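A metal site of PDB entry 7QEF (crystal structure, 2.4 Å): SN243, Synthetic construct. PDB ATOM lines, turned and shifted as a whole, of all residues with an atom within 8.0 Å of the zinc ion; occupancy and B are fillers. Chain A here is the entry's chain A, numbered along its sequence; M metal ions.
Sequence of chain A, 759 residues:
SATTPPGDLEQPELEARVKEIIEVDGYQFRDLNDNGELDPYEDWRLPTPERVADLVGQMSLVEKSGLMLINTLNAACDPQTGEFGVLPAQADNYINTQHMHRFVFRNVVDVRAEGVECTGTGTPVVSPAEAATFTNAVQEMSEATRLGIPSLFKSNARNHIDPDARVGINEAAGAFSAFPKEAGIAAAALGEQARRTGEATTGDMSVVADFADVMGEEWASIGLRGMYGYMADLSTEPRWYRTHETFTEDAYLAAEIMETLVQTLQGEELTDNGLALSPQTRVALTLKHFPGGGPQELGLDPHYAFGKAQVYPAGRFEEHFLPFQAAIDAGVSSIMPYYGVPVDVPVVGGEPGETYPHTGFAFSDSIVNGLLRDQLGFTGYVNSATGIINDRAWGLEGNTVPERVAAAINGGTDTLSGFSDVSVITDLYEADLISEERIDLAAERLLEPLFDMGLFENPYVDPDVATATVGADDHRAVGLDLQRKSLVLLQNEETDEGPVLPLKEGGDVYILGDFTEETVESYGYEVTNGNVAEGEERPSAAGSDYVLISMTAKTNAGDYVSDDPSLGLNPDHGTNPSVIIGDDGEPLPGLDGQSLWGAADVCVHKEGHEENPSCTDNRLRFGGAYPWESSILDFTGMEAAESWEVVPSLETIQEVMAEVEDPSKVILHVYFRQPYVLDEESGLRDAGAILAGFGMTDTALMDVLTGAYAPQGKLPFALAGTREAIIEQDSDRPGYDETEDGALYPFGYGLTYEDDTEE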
ATOM      1  N   GLU A  20       0.337  24.360  12.019  1.00  0.00           N
ATOM      2  CA  GLU A  20      -1.008  24.829  12.454  1.00  0.00           C
ATOM      3  C   GLU A  20      -1.792  23.718  13.143  1.00  0.00           C
ATOM      4  O   GLU A  20      -1.338  22.564  13.136  1.00  0.00           O
ATOM      5  CB  GLU A  20      -1.785  25.394  11.261  1.00  0.00           C
ATOM      6  CG  GLU A  20      -1.456  26.842  10.979  1.00  0.00           C
ATOM      7  CD  GLU A  20      -1.671  27.771  12.168  1.00  0.00           C
ATOM      8  OE1 GLU A  20      -2.495  27.425  13.043  1.00  0.00           O
ATOM      9  OE2 GLU A  20      -1.017  28.823  12.231  1.00  0.00           O
ATOM     10  N   ILE A  22      -5.205  21.315  13.651  1.00  0.00           N
ATOM     11  CA  ILE A  22      -6.282  20.719  12.809  1.00  0.00           C
ATOM     12  C   ILE A  22      -7.345  20.126  13.740  1.00  0.00           C
ATOM     13  O   ILE A  22      -6.962  19.447  14.718  1.00  0.00           O
ATOM     14  CB  ILE A  22      -5.691  19.664  11.856  1.00  0.00           C
ATOM     15  CG1 ILE A  22      -5.148  18.450  12.620  1.00  0.00           C
ATOM     16  CG2 ILE A  22      -4.636  20.285  10.961  1.00  0.00           C
ATOM     17  CD1 ILE A  22      -4.556  17.392  11.728  1.00  0.00           C
ATOM     18  N   ARG A  30      -2.175  19.030  16.528  1.00  0.00           N
ATOM     19  CA  ARG A  30      -1.116  19.803  15.822  1.00  0.00           C
ATOM     20  C   ARG A  30      -0.686  19.037  14.572  1.00  0.00           C
ATOM     21  O   ARG A  30      -0.242  17.879  14.716  1.00  0.00           O
ATOM     22  CB  ARG A  30       0.079  20.052  16.744  1.00  0.00           C
ATOM     23  CG  ARG A  30      -0.234  20.910  17.960  1.00  0.00           C
ATOM     24  CD  ARG A  30       0.988  21.704  18.386  1.00  0.00           C
ATOM     25  NE  ARG A  30       2.132  20.858  18.703  1.00  0.00           N
ATOM     26  CZ  ARG A  30       3.376  21.289  18.784  1.00  0.00           C
ATOM     27  NH1 ARG A  30       4.352  20.449  19.075  1.00  0.00           N
ATOM     28  NH2 ARG A  30       3.657  22.565  18.555  1.00  0.00           N
ATOM     29  N   ASP A  31      -0.796  19.664  13.406  1.00  0.00           N
ATOM     30  CA  ASP A  31      -0.340  19.018  12.163  1.00  0.00           C
ATOM     31  C   ASP A  31       1.133  19.324  11.968  1.00  0.00           C
ATOM     32  O   ASP A  31       1.512  20.310  11.337  1.00  0.00           O
ATOM     33  CB  ASP A  31      -1.155  19.479  10.958  1.00  0.00           C
ATOM     34  CG  ASP A  31      -0.919  18.594   9.736  1.00  0.00           C
ATOM     35  OD1 ASP A  31      -0.491  17.447   9.927  1.00  0.00           O
ATOM     36  OD2 ASP A  31      -1.139  19.048   8.598  1.00  0.00           O
ATOM     37  N   LEU A  32       1.966  18.413  12.457  1.00  0.00           N
ATOM     38  CA  LEU A  32       3.395  18.668  12.534  1.00  0.00           C
ATOM     39  C   LEU A  32       4.144  18.306  11.268  1.00  0.00           C
ATOM     40  O   LEU A  32       5.175  18.943  10.972  1.00  0.00           O
ATOM     41  CB  LEU A  32       3.983  17.922  13.740  1.00  0.00           C
ATOM     42  CG  LEU A  32       3.438  18.481  15.064  1.00  0.00           C
ATOM     43  CD1 LEU A  32       3.650  17.523  16.236  1.00  0.00           C
ATOM     44  CD2 LEU A  32       4.033  19.864  15.396  1.00  0.00           C
ATOM     45  N   ASN A  33       3.658  17.309  10.500  1.00  0.00           N
ATOM     46  CA  ASN A  33       4.205  17.041   9.168  1.00  0.00           C
ATOM     47  C   ASN A  33       3.693  18.023   8.139  1.00  0.00           C
ATOM     48  O   ASN A  33       4.212  18.025   7.014  1.00  0.00           O
ATOM     49  CB  ASN A  33       3.904  15.625   8.678  1.00  0.00           C
ATOM     50  CG  ASN A  33       2.467  15.238   8.858  1.00  0.00           C
ATOM     51  OD1 ASN A  33       1.576  16.089   8.784  1.00  0.00           O
ATOM     52  ND2 ASN A  33       2.221  13.943   9.037  1.00  0.00           N
ATOM     53  N   ASP A  34       2.678  18.832   8.469  1.00  0.00           N
ATOM     54  CA  ASP A  34       2.137  19.841   7.567  1.00  0.00           C
ATOM     55  C   ASP A  34       1.663  19.201   6.270  1.00  0.00           C
ATOM     56  O   ASP A  34       1.882  19.711   5.172  1.00  0.00           O
ATOM     57  CB  ASP A  34       3.178  20.954   7.337  1.00  0.00           C
ATOM     58  CG  ASP A  34       2.699  22.069   6.426  1.00  0.00           C
ATOM     59  OD1 ASP A  34       1.842  22.910   6.813  1.00  0.00           O
ATOM     60  OD2 ASP A  34       3.226  22.102   5.293  1.00  0.00           O
ATOM     61  N   ASN A  35       0.981  18.056   6.437  1.00  0.00           N
ATOM     62  CA  ASN A  35       0.411  17.310   5.294  1.00  0.00           C
ATOM     63  C   ASN A  35      -1.071  17.654   5.188  1.00  0.00           C
ATOM     64  O   ASN A  35      -1.681  17.362   4.152  1.00  0.00           O
ATOM     65  CB  ASN A  35       0.540  15.802   5.494  1.00  0.00           C
ATOM     66  CG  ASN A  35      -0.211  15.299   6.707  1.00  0.00           C
ATOM     67  OD1 ASN A  35      -0.766  16.085   7.474  1.00  0.00           O
ATOM     68  ND2 ASN A  35      -0.231  13.989   6.898  1.00  0.00           N
ATOM     69  N   GLY A  36      -1.635  18.246   6.247  1.00  0.00           N
ATOM     70  CA  GLY A  36      -3.045  18.646   6.251  1.00  0.00           C
ATOM     71  C   GLY A  36      -3.918  17.559   6.839  1.00  0.00           C
ATOM     72  O   GLY A  36      -5.151  17.730   6.848  1.00  0.00           O
ATOM     73  N   GLU A  37      -3.309  16.475   7.302  1.00  0.00           N
ATOM     74  CA  GLU A  37      -4.116  15.337   7.810  1.00  0.00           C
ATOM     75  C   GLU A  37      -3.574  14.900   9.171  1.00  0.00           C
ATOM     76  O   GLU A  37      -2.397  15.167   9.464  1.00  0.00           O
ATOM     77  CB  GLU A  37      -4.095  14.186   6.803  1.00  0.00           C
ATOM     78  CG  GLU A  37      -5.279  13.255   6.945  1.00  0.00           C
ATOM     79  CD  GLU A  37      -5.531  12.353   5.752  1.00  0.00           C
ATOM     80  OE1 GLU A  37      -4.614  12.207   4.928  1.00  0.00           O
ATOM     81  OE2 GLU A  37      -6.645  11.808   5.652  1.00  0.00           O
ATOM     82  N   LEU A  38      -4.428  14.252   9.974  1.00  0.00           N
ATOM     83  CA  LEU A  38      -3.998  13.811  11.317  1.00  0.00           C
ATOM     84  C   LEU A  38      -3.241  12.495  11.184  1.00  0.00           C
ATOM     85  O   LEU A  38      -3.841  11.512  10.726  1.00  0.00           O
ATOM     86  CB  LEU A  38      -5.238  13.621  12.205  1.00  0.00           C
ATOM     87  CG  LEU A  38      -4.956  13.030  13.590  1.00  0.00           C
ATOM     88  CD1 LEU A  38      -3.999  13.908  14.376  1.00  0.00           C
ATOM     89  CD2 LEU A  38      -6.248  12.828  14.359  1.00  0.00           C
ATOM     90  N   ASP A  39      -1.967  12.483  11.588  1.00  0.00           N
ATOM     91  CA  ASP A  39      -1.206  11.211  11.585  1.00  0.00           C
ATOM     92  C   ASP A  39      -1.275  10.632  12.993  1.00  0.00           C
ATOM     93  O   ASP A  39      -1.362  11.420  13.952  1.00  0.00           O
ATOM     94  CB  ASP A  39       0.208  11.423  11.043  1.00  0.00           C
ATOM     95  CG  ASP A  39       0.244  12.138   9.715  1.00  0.00           C
ATOM     96  OD1 ASP A  39      -0.318  13.249   9.628  1.00  0.00           O
ATOM     97  OD2 ASP A  39       0.827  11.584   8.771  1.00  0.00           O
ATOM     98  N   PRO A  40      -1.282   9.290  13.161  1.00  0.00           N
ATOM     99  CA  PRO A  40      -1.434   8.701  14.484  1.00  0.00           C
ATOM    100  C   PRO A  40      -0.450   9.276  15.515  1.00  0.00           C
ATOM    101  O   PRO A  40      -0.784   9.292  16.683  1.00  0.00           O
ATOM    102  CB  PRO A  40      -1.127   7.215  14.223  1.00  0.00           C
ATOM    103  CG  PRO A  40      -1.539   7.009  12.780  1.00  0.00           C
ATOM    104  CD  PRO A  40      -1.184   8.303  12.094  1.00  0.00           C
ATOM    105  N   TYR A  41       0.730   9.721  15.082  1.00  0.00           N
ATOM    106  CA  TYR A  41       1.744  10.253  16.018  1.00  0.00           C
ATOM    107  C   TYR A  41       1.310  11.647  16.495  1.00  0.00           C
ATOM    108  O   TYR A  41       1.668  12.015  17.626  1.00  0.00           O
ATOM    109  CB  TYR A  41       3.141  10.242  15.378  1.00  0.00           C
ATOM    110  CG  TYR A  41       3.558  11.480  14.629  1.00  0.00           C
ATOM    111  CD1 TYR A  41       4.103  12.568  15.288  1.00  0.00           C
ATOM    112  CD2 TYR A  41       3.456  11.556  13.241  1.00  0.00           C
ATOM    113  CE1 TYR A  41       4.508  13.700  14.603  1.00  0.00           C
ATOM    114  CE2 TYR A  41       3.858  12.683  12.547  1.00  0.00           C
ATOM    115  CZ  TYR A  41       4.391  13.758  13.230  1.00  0.00           C
ATOM    116  OH  TYR A  41       4.785  14.877  12.544  1.00  0.00           O
ATOM    117  N   GLU A  42       0.556  12.364  15.666  1.00  0.00           N
ATOM    118  CA  GLU A  42       0.044  13.707  16.044  1.00  0.00           C
ATOM    119  C   GLU A  42      -1.243  13.551  16.858  1.00  0.00           C
ATOM    120  O   GLU A  42      -1.754  14.566  17.348  1.00  0.00           O
ATOM    121  CB  GLU A  42      -0.183  14.524  14.777  1.00  0.00           C
ATOM    122  CG  GLU A  42       1.034  14.643  13.889  1.00  0.00           C
ATOM    123  CD  GLU A  42       0.773  15.216  12.506  1.00  0.00           C
ATOM    124  OE1 GLU A  42      -0.367  15.114  12.036  1.00  0.00           O
ATOM    125  OE2 GLU A  42       1.719  15.756  11.912  1.00  0.00           O
ATOM    126  N   ASP A  54       4.327   5.257  14.498  1.00  0.00           N
ATOM    127  CA  ASP A  54       3.962   6.042  13.322  1.00  0.00           C
ATOM    128  C   ASP A  54       4.997   7.117  13.019  1.00  0.00           C
ATOM    129  O   ASP A  54       5.272   7.419  11.850  1.00  0.00           O
ATOM    130  CB  ASP A  54       2.582   6.679  13.495  1.00  0.00           C
ATOM    131  CG  ASP A  54       2.090   7.356  12.234  1.00  0.00           C
ATOM    132  OD1 ASP A  54       1.734   6.626  11.281  1.00  0.00           O
ATOM    133  OD2 ASP A  54       2.083   8.607  12.182  1.00  0.00           O
ATOM    134  N   GLN A  58       7.816   7.151   9.622  1.00  0.00           N
ATOM    135  CA  GLN A  58       7.948   8.215   8.640  1.00  0.00           C
ATOM    136  C   GLN A  58       9.308   8.870   8.590  1.00  0.00           C
ATOM    137  O   GLN A  58       9.495   9.805   7.805  1.00  0.00           O
ATOM    138  CB  GLN A  58       6.934   9.331   8.929  1.00  0.00           C
ATOM    139  CG  GLN A  58       5.503   8.920   9.036  1.00  0.00           C
ATOM    140  CD  GLN A  58       4.624  10.062   9.467  1.00  0.00           C
ATOM    141  OE1 GLN A  58       4.876  11.218   9.100  1.00  0.00           O
ATOM    142  NE2 GLN A  58       3.594   9.764  10.232  1.00  0.00           N
HETATM  143 ZN    ZN M   1      -0.214  15.525   9.754  1.00  0.00          ZN
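The side-chain hydroxyl (OH) of Tyr 41 lies within hydrogen-bond range of the backbone NH (N) of Asn 33 (3.4 Å).
The side-chain carboxylate of Asp 31 sits at hydrogen-bond distance from the backbone NH of Gly 36, 2.5 Å away.
N of Asp 31 is in hydrogen-bond range of O of Glu 20, at 3.0 Å.
OE2 of Glu 42 sits at hydrogen-bond distance from OH of Tyr 41.
OE2 of Glu 42 lies within hydrogen-bond range of N of Leu 32, at 2.7 Å.
Six residues have an atom within 4 Å of the zinc ion: Asp 31, Asn 33, Asn 35, Glu 37, Asp 39 and Glu 42.
The nearest printed residue that does not touch the zinc ion is Leu 38 (4.4 Å).
The zinc ion is bound by OD1 of Asp 31 (1.9 Å), OD1 of Asn 33 (2.1 Å), O of Glu 37 (2.2 Å), OD1 of Asp 39 (2.3 Å), OE1 of Glu 42 (2.3 Å) and OD1 of Asn 35 (2.4 Å).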
